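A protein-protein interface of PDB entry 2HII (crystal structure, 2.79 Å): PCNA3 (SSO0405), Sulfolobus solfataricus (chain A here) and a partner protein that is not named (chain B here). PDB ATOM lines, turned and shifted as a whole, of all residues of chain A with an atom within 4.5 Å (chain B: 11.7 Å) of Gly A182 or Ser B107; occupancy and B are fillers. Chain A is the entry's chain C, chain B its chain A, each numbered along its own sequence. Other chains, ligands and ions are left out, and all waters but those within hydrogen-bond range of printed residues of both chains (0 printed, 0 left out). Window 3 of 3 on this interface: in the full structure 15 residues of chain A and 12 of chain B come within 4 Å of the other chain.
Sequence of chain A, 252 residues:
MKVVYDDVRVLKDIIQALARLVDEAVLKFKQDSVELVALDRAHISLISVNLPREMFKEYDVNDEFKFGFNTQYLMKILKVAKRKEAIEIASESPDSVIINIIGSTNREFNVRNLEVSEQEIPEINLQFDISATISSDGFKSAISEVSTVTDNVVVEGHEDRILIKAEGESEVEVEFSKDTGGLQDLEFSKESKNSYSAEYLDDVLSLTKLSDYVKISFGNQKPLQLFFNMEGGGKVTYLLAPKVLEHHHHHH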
ATOM      1  N   THR A 133       1.547 -26.038  -9.603  1.00  0.00           N
ATOM      2  CA  THR A 133       2.280 -25.887  -8.346  1.00  0.00           C
ATOM      3  C   THR A 133       3.792 -25.715  -8.545  1.00  0.00           C
ATOM      4  O   THR A 133       4.478 -26.632  -8.989  1.00  0.00           O
ATOM      5  CB  THR A 133       2.019 -27.066  -7.391  1.00  0.00           C
ATOM      6  OG1 THR A 133       0.603 -27.281  -7.261  1.00  0.00           O
ATOM      7  CG2 THR A 133       2.623 -26.776  -6.021  1.00  0.00           C
ATOM      8  N   ILE A 134       4.292 -24.531  -8.194  1.00  0.00           N
ATOM      9  CA  ILE A 134       5.725 -24.229  -8.224  1.00  0.00           C
ATOM     10  C   ILE A 134       6.178 -23.713  -6.877  1.00  0.00           C
ATOM     11  O   ILE A 134       5.348 -23.456  -5.993  1.00  0.00           O
ATOM     12  CB  ILE A 134       6.072 -23.131  -9.252  1.00  0.00           C
ATOM     13  CG1 ILE A 134       5.340 -21.832  -8.924  1.00  0.00           C
ATOM     14  CG2 ILE A 134       5.738 -23.583 -10.651  1.00  0.00           C
ATOM     15  CD1 ILE A 134       6.079 -20.592  -9.325  1.00  0.00           C
ATOM     16  N   SER A 135       7.488 -23.521  -6.738  1.00  0.00           N
ATOM     17  CA  SER A 135       8.057 -23.033  -5.487  1.00  0.00           C
ATOM     18  C   SER A 135       7.727 -21.568  -5.224  1.00  0.00           C
ATOM     19  O   SER A 135       7.746 -20.729  -6.138  1.00  0.00           O
ATOM     20  CB  SER A 135       9.562 -23.266  -5.435  1.00  0.00           C
ATOM     21  OG  SER A 135      10.295 -22.096  -5.699  1.00  0.00           O
ATOM     22  N   GLY A 138      10.533 -19.267  -6.036  1.00  0.00           N
ATOM     23  CA  GLY A 138      10.456 -19.133  -7.480  1.00  0.00           C
ATOM     24  C   GLY A 138       9.398 -18.145  -7.913  1.00  0.00           C
ATOM     25  O   GLY A 138       9.659 -17.280  -8.747  1.00  0.00           O
ATOM     26  N   PHE A 176       8.458 -22.006 -15.696  1.00  0.00           N
ATOM     27  CA  PHE A 176       8.544 -23.198 -14.885  1.00  0.00           C
ATOM     28  C   PHE A 176       7.996 -24.351 -15.719  1.00  0.00           C
ATOM     29  O   PHE A 176       6.821 -24.338 -16.101  1.00  0.00           O
ATOM     30  CB  PHE A 176       7.755 -23.044 -13.580  1.00  0.00           C
ATOM     31  CG  PHE A 176       8.151 -21.852 -12.743  1.00  0.00           C
ATOM     32  CD1 PHE A 176       7.486 -20.637 -12.872  1.00  0.00           C
ATOM     33  CD2 PHE A 176       9.159 -21.951 -11.793  1.00  0.00           C
ATOM     34  CE1 PHE A 176       7.845 -19.530 -12.083  1.00  0.00           C
ATOM     35  CE2 PHE A 176       9.515 -20.840 -11.001  1.00  0.00           C
ATOM     36  CZ  PHE A 176       8.857 -19.635 -11.152  1.00  0.00           C
ATOM     37  N   SER A 177       8.855 -25.328 -16.009  1.00  0.00           N
ATOM     38  CA  SER A 177       8.501 -26.467 -16.864  1.00  0.00           C
ATOM     39  C   SER A 177       8.470 -27.749 -16.044  1.00  0.00           C
ATOM     40  O   SER A 177       8.945 -27.764 -14.912  1.00  0.00           O
ATOM     41  CB  SER A 177       9.512 -26.653 -18.014  1.00  0.00           C
ATOM     42  OG  SER A 177      10.440 -25.585 -18.136  1.00  0.00           O
ATOM     43  N   THR A 180      12.213 -29.091 -16.479  1.00  0.00           N
ATOM     44  CA  THR A 180      13.102 -28.211 -15.719  1.00  0.00           C
ATOM     45  C   THR A 180      13.078 -28.578 -14.229  1.00  0.00           C
ATOM     46  O   THR A 180      13.945 -28.150 -13.462  1.00  0.00           O
ATOM     47  CB  THR A 180      12.723 -26.691 -15.953  1.00  0.00           C
ATOM     48  OG1 THR A 180      13.900 -25.898 -16.135  1.00  0.00           O
ATOM     49  CG2 THR A 180      11.876 -26.088 -14.815  1.00  0.00           C
ATOM     50  N   GLY A 181      12.081 -29.380 -13.838  1.00  0.00           N
ATOM     51  CA  GLY A 181      11.833 -29.742 -12.436  1.00  0.00           C
ATOM     52  C   GLY A 181      11.223 -28.597 -11.640  1.00  0.00           C
ATOM     53  O   GLY A 181      11.018 -28.709 -10.429  1.00  0.00           O
ATOM     54  N   GLY A 182      10.934 -27.488 -12.318  1.00  0.00           N
ATOM     55  CA  GLY A 182      10.419 -26.298 -11.662  1.00  0.00           C
ATOM     56  C   GLY A 182       8.939 -26.407 -11.383  1.00  0.00           C
ATOM     57  O   GLY A 182       8.460 -25.958 -10.346  1.00  0.00           O
ATOM     58  N   LEU A 183       8.215 -27.002 -12.319  1.00  0.00           N
ATOM     59  CA  LEU A 183       6.779 -27.179 -12.206  1.00  0.00           C
ATOM     60  C   LEU A 183       6.497 -28.523 -11.528  1.00  0.00           C
ATOM     61  O   LEU A 183       6.570 -29.588 -12.154  1.00  0.00           O
ATOM     62  CB  LEU A 183       6.159 -27.077 -13.604  1.00  0.00           C
ATOM     63  CG  LEU A 183       4.675 -27.153 -13.955  1.00  0.00           C
ATOM     64  CD1 LEU A 183       4.313 -28.547 -14.393  1.00  0.00           C
ATOM     65  CD2 LEU A 183       3.815 -26.694 -12.814  1.00  0.00           C
ATOM     66  N   GLN A 184       6.188 -28.464 -10.235  1.00  0.00           N
ATOM     67  CA  GLN A 184       6.004 -29.664  -9.431  1.00  0.00           C
ATOM     68  C   GLN A 184       4.704 -30.416  -9.720  1.00  0.00           C
ATOM     69  O   GLN A 184       4.655 -31.632  -9.589  1.00  0.00           O
ATOM     70  CB  GLN A 184       6.151 -29.346  -7.944  1.00  0.00           C
ATOM     71  CG  GLN A 184       5.404 -30.306  -7.042  1.00  0.00           C
ATOM     72  CD  GLN A 184       6.237 -30.791  -5.870  1.00  0.00           C
ATOM     73  OE1 GLN A 184       5.956 -30.444  -4.712  1.00  0.00           O
ATOM     74  NE2 GLN A 184       7.268 -31.603  -6.158  1.00  0.00           N
ATOM     75  N   LYS B  10      25.885 -13.664 -11.596  1.00  0.00           N
ATOM     76  CA  LYS B  10      26.208 -12.556 -10.705  1.00  0.00           C
ATOM     77  C   LYS B  10      27.573 -11.975 -11.060  1.00  0.00           C
ATOM     78  O   LYS B  10      27.682 -10.770 -11.293  1.00  0.00           O
ATOM     79  CB  LYS B  10      26.106 -12.934  -9.223  1.00  0.00           C
ATOM     80  CG  LYS B  10      24.666 -13.209  -8.734  1.00  0.00           C
ATOM     81  CD  LYS B  10      23.746 -11.976  -8.849  1.00  0.00           C
ATOM     82  CE  LYS B  10      22.259 -12.347  -8.931  1.00  0.00           C
ATOM     83  NZ  LYS B  10      21.706 -12.757  -7.612  1.00  0.00           N
ATOM     84  N   LYS B  81      16.736  -8.570  -8.852  1.00  0.00           N
ATOM     85  CA  LYS B  81      15.587  -9.238  -8.238  1.00  0.00           C
ATOM     86  C   LYS B  81      15.647 -10.748  -8.450  1.00  0.00           C
ATOM     87  O   LYS B  81      14.822 -11.495  -7.904  1.00  0.00           O
ATOM     88  CB  LYS B  81      14.269  -8.658  -8.778  1.00  0.00           C
ATOM     89  CG  LYS B  81      13.610  -7.622  -7.852  1.00  0.00           C
ATOM     90  CD  LYS B  81      14.346  -6.270  -7.791  1.00  0.00           C
ATOM     91  CE  LYS B  81      14.218  -5.613  -6.407  1.00  0.00           C
ATOM     92  NZ  LYS B  81      12.820  -5.649  -5.833  1.00  0.00           N
ATOM     93  N   ALA B  82      16.621 -11.188  -9.250  1.00  0.00           N
ATOM     94  CA  ALA B  82      16.886 -12.617  -9.416  1.00  0.00           C
ATOM     95  C   ALA B  82      17.717 -13.080  -8.229  1.00  0.00           C
ATOM     96  O   ALA B  82      18.957 -13.034  -8.247  1.00  0.00           O
ATOM     97  CB  ALA B  82      17.592 -12.902 -10.722  1.00  0.00           C
ATOM     98  N   SER B  83      17.007 -13.474  -7.174  1.00  0.00           N
ATOM     99  CA  SER B  83      17.629 -14.009  -5.974  1.00  0.00           C
ATOM    100  C   SER B  83      18.292 -15.311  -6.413  1.00  0.00           C
ATOM    101  O   SER B  83      17.629 -16.362  -6.572  1.00  0.00           O
ATOM    102  CB  SER B  83      16.579 -14.242  -4.877  1.00  0.00           C
ATOM    103  OG  SER B  83      17.183 -14.640  -3.657  1.00  0.00           O
ATOM    104  N   SER B  84      19.593 -15.228  -6.666  1.00  0.00           N
ATOM    105  CA  SER B  84      20.285 -16.353  -7.260  1.00  0.00           C
ATOM    106  C   SER B  84      21.721 -16.452  -6.794  1.00  0.00           C
ATOM    107  O   SER B  84      22.383 -15.445  -6.509  1.00  0.00           O
ATOM    108  CB  SER B  84      20.178 -16.289  -8.786  1.00  0.00           C
ATOM    109  OG  SER B  84      18.838 -16.568  -9.201  1.00  0.00           O
ATOM    110  N   LYS B  85      22.180 -17.692  -6.713  1.00  0.00           N
ATOM    111  CA  LYS B  85      23.462 -18.001  -6.136  1.00  0.00           C
ATOM    112  C   LYS B  85      24.427 -18.294  -7.268  1.00  0.00           C
ATOM    113  O   LYS B  85      25.246 -17.453  -7.620  1.00  0.00           O
ATOM    114  CB  LYS B  85      23.297 -19.204  -5.201  1.00  0.00           C
ATOM    115  CG  LYS B  85      22.495 -18.864  -3.951  1.00  0.00           C
ATOM    116  CD  LYS B  85      21.349 -19.834  -3.687  1.00  0.00           C
ATOM    117  CE  LYS B  85      20.536 -19.362  -2.459  1.00  0.00           C
ATOM    118  NZ  LYS B  85      19.354 -20.213  -2.128  1.00  0.00           N
ATOM    119  N   LYS B  86      24.249 -19.458  -7.881  1.00  0.00           N
ATOM    120  CA  LYS B  86      25.257 -20.108  -8.700  1.00  0.00           C
ATOM    121  C   LYS B  86      24.892 -20.118 -10.185  1.00  0.00           C
ATOM    122  O   LYS B  86      25.650 -20.649 -11.007  1.00  0.00           O
ATOM    123  CB  LYS B  86      25.368 -21.557  -8.211  1.00  0.00           C
ATOM    124  CG  LYS B  86      26.728 -22.230  -8.396  1.00  0.00           C
ATOM    125  CD  LYS B  86      26.741 -23.628  -7.747  1.00  0.00           C
ATOM    126  CE  LYS B  86      26.703 -23.560  -6.199  1.00  0.00           C
ATOM    127  NZ  LYS B  86      26.830 -24.899  -5.541  1.00  0.00           N
ATOM    128  N   ALA B  87      23.734 -19.539 -10.514  1.00  0.00           N
ATOM    129  CA  ALA B  87      23.153 -19.562 -11.868  1.00  0.00           C
ATOM    130  C   ALA B  87      24.116 -19.195 -13.001  1.00  0.00           C
ATOM    131  O   ALA B  87      24.943 -18.304 -12.863  1.00  0.00           O
ATOM    132  CB  ALA B  87      21.919 -18.670 -11.923  1.00  0.00           C
ATOM    133  N   THR B  88      23.990 -19.891 -14.124  1.00  0.00           N
ATOM    134  CA  THR B  88      24.836 -19.655 -15.273  1.00  0.00           C
ATOM    135  C   THR B  88      24.189 -18.558 -16.151  1.00  0.00           C
ATOM    136  O   THR B  88      23.026 -18.221 -15.936  1.00  0.00           O
ATOM    137  CB  THR B  88      25.048 -20.962 -16.030  1.00  0.00           C
ATOM    138  OG1 THR B  88      26.057 -20.770 -17.017  1.00  0.00           O
ATOM    139  CG2 THR B  88      23.753 -21.429 -16.698  1.00  0.00           C
ATOM    140  N   ILE B 102      18.870 -16.817 -17.913  1.00  0.00           N
ATOM    141  CA  ILE B 102      19.393 -17.262 -16.623  1.00  0.00           C
ATOM    142  C   ILE B 102      18.541 -18.412 -16.104  1.00  0.00           C
ATOM    143  O   ILE B 102      17.320 -18.418 -16.294  1.00  0.00           O
ATOM    144  CB  ILE B 102      19.311 -16.134 -15.582  1.00  0.00           C
ATOM    145  CG1 ILE B 102      19.964 -14.851 -16.102  1.00  0.00           C
ATOM    146  CG2 ILE B 102      19.951 -16.543 -14.291  1.00  0.00           C
ATOM    147  CD1 ILE B 102      18.967 -13.845 -16.660  1.00  0.00           C
ATOM    148  N   ARG B 103      19.172 -19.376 -15.436  1.00  0.00           N
ATOM    149  CA  ARG B 103      18.435 -20.500 -14.864  1.00  0.00           C
ATOM    150  C   ARG B 103      18.768 -20.688 -13.389  1.00  0.00           C
ATOM    151  O   ARG B 103      19.941 -20.774 -13.025  1.00  0.00           O
ATOM    152  CB  ARG B 103      18.739 -21.767 -15.655  1.00  0.00           C
ATOM    153  CG  ARG B 103      18.686 -21.559 -17.164  1.00  0.00           C
ATOM    154  CD  ARG B 103      19.896 -22.168 -17.848  1.00  0.00           C
ATOM    155  NE  ARG B 103      19.930 -21.911 -19.290  1.00  0.00           N
ATOM    156  CZ  ARG B 103      19.288 -22.635 -20.203  1.00  0.00           C
ATOM    157  NH1 ARG B 103      18.524 -23.656 -19.829  1.00  0.00           N
ATOM    158  NH2 ARG B 103      19.399 -22.331 -21.489  1.00  0.00           N
ATOM    159  N   ASP B 104      17.742 -20.738 -12.543  1.00  0.00           N
ATOM    160  CA  ASP B 104      17.951 -20.951 -11.123  1.00  0.00           C
ATOM    161  C   ASP B 104      17.731 -22.425 -10.805  1.00  0.00           C
ATOM    162  O   ASP B 104      16.729 -23.019 -11.217  1.00  0.00           O
ATOM    163  CB  ASP B 104      17.054 -20.028 -10.284  1.00  0.00           C
ATOM    164  CG  ASP B 104      17.460 -19.980  -8.789  1.00  0.00           C
ATOM    165  OD1 ASP B 104      17.171 -20.969  -8.044  1.00  0.00           O
ATOM    166  OD2 ASP B 104      18.040 -18.933  -8.357  1.00  0.00           O
ATOM    167  N   GLU B 105      18.688 -23.006 -10.079  1.00  0.00           N
ATOM    168  CA  GLU B 105      18.728 -24.446  -9.793  1.00  0.00           C
ATOM    169  C   GLU B 105      17.677 -24.860  -8.776  1.00  0.00           C
ATOM    170  O   GLU B 105      16.974 -25.854  -8.966  1.00  0.00           O
ATOM    171  CB  GLU B 105      20.137 -24.857  -9.317  1.00  0.00           C
ATOM    172  CG  GLU B 105      20.237 -26.137  -8.437  1.00  0.00           C
ATOM    173  CD  GLU B 105      19.848 -27.434  -9.163  1.00  0.00           C
ATOM    174  OE1 GLU B 105      19.041 -28.227  -8.603  1.00  0.00           O
ATOM    175  OE2 GLU B 105      20.352 -27.660 -10.288  1.00  0.00           O
ATOM    176  N   LYS B 106      17.578 -24.096  -7.695  1.00  0.00           N
ATOM    177  CA  LYS B 106      16.706 -24.466  -6.584  1.00  0.00           C
ATOM    178  C   LYS B 106      15.225 -24.341  -6.940  1.00  0.00           C
ATOM    179  O   LYS B 106      14.399 -25.102  -6.427  1.00  0.00           O
ATOM    180  CB  LYS B 106      17.042 -23.630  -5.334  1.00  0.00           C
ATOM    181  N   SER B 107      14.907 -23.386  -7.821  1.00  0.00           N
ATOM    182  CA  SER B 107      13.521 -23.067  -8.190  1.00  0.00           C
ATOM    183  C   SER B 107      13.113 -23.594  -9.562  1.00  0.00           C
ATOM    184  O   SER B 107      11.937 -23.911  -9.788  1.00  0.00           O
ATOM    185  CB  SER B 107      13.285 -21.554  -8.128  1.00  0.00           C
ATOM    186  OG  SER B 107      14.207 -20.835  -8.927  1.00  0.00           O
ATOM    187  N   GLY B 108      14.084 -23.678 -10.469  1.00  0.00           N
ATOM    188  CA  GLY B 108      13.849 -24.195 -11.817  1.00  0.00           C
ATOM    189  C   GLY B 108      13.437 -23.106 -12.785  1.00  0.00           C
ATOM    190  O   GLY B 108      13.084 -23.380 -13.937  1.00  0.00           O
ATOM    191  N   ALA B 109      13.517 -21.868 -12.305  1.00  0.00           N
ATOM    192  CA  ALA B 109      13.020 -20.701 -12.998  1.00  0.00           C
ATOM    193  C   ALA B 109      13.952 -20.242 -14.115  1.00  0.00           C
ATOM    194  O   ALA B 109      15.001 -19.665 -13.852  1.00  0.00           O
ATOM    195  CB  ALA B 109      12.808 -19.580 -11.988  1.00  0.00           C
ATOM    196  N   LYS B 110      13.556 -20.483 -15.361  1.00  0.00           N
ATOM    197  CA  LYS B 110      14.285 -19.978 -16.521  1.00  0.00           C
ATOM    198  C   LYS B 110      13.753 -18.598 -16.885  1.00  0.00           C
ATOM    199  O   LYS B 110      12.695 -18.459 -17.487  1.00  0.00           O
ATOM    200  CB  LYS B 110      14.169 -20.971 -17.692  1.00  0.00           C
ATOM    201  CG  LYS B 110      14.805 -20.548 -19.019  1.00  0.00           C
ATOM    202  CD  LYS B 110      15.146 -21.765 -19.898  1.00  0.00           C
ATOM    203  CE  LYS B 110      13.947 -22.365 -20.650  1.00  0.00           C
ATOM    204  NZ  LYS B 110      13.748 -21.765 -21.992  1.00  0.00           N
ATOM    205  N   SER B 111      14.481 -17.571 -16.483  1.00  0.00           N
ATOM    206  CA  SER B 111      14.157 -16.216 -16.902  1.00  0.00           C
ATOM    207  C   SER B 111      14.990 -15.813 -18.110  1.00  0.00           C
ATOM    208  O   SER B 111      16.223 -15.740 -18.048  1.00  0.00           O
ATOM    209  CB  SER B 111      14.303 -15.206 -15.763  1.00  0.00           C
ATOM    210  OG  SER B 111      15.105 -15.702 -14.714  1.00  0.00           O
ATOM    211  N   THR B 112      14.294 -15.574 -19.218  1.00  0.00           N
ATOM    212  CA  THR B 112      14.938 -15.160 -20.446  1.00  0.00           C
ATOM    213  C   THR B 112      14.610 -13.694 -20.677  1.00  0.00           C
ATOM    214  O   THR B 112      13.450 -13.303 -20.599  1.00  0.00           O
ATOM    215  CB  THR B 112      14.540 -16.048 -21.674  1.00  0.00           C
ATOM    216  OG1 THR B 112      13.441 -15.465 -22.371  1.00  0.00           O
ATOM    217  CG2 THR B 112      14.178 -17.482 -21.258  1.00  0.00           C
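The backbone carbonyl oxygen (O) of Gly B108 sits close to the side-chain hydroxyl (OG1) of Thr A180, 3.4 Å away.
The side-chain carboxylate (OD1) of Asp B104 is in hydrogen-bond range of the side-chain hydroxyl (OG) of Ser B107, at 3.1 Å.
O of Ala B109 is in hydrogen-bond range of N of Asp B104 (3.2 Å).
OG of Ser A135 lies within hydrogen-bond range of N of Gly A138 (2.9 Å).
The backbone NH (N) of Gly A182 is in hydrogen-bond range of the backbone carbonyl oxygen (O) of Ser A177.
Among the printed residues, pairs that only touch across the chains: Ser A135 with Ser B107, Gly A138 with Ser B107, Phe A176 with Ser B107, Phe A176 with Ala B109 and Gly A182 with Ser B107.
Gly A182 touches just one residue of chain B: Ser B107 (3.4 Å).
Of chain A, only Ser A135, Gly A138, Phe A176 and Gly A182 come within 4 Å of Ser B107.
No residue of chain B comes within 4 Å of Ile A134.
Of chain B, only Ser B107 comes within 4 Å of Ser A135.
No residue of chain B comes within 4 Å of Ser A177.
Thr A180 touches just one residue of chain B: Gly B108.
No residue of chain B comes within 4 Å of Gly A181.
No residue of chain B comes within 4 Å of Leu A183.
Of the printed residues of chain A, Ala B109 touches Phe A176.
Printed residues of chain A within 4 Å of Gly B108: Thr A180.
Lys B85 touches none of the printed residues of chain A.
Ser B83 touches none of the printed residues of chain A.
The nearest residue of chain B that does not touch Gly A182 is Gly B108 (4.03 Å).
The nearest printed residue of chain A that does not touch Ser B107 is Gly A181 (4.9 Å).
Of the 20 printed residues of chain B, 3 touch a printed residue of chain A.
Of the 11 printed residues of chain A, 5 touch a printed residue of chain B.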
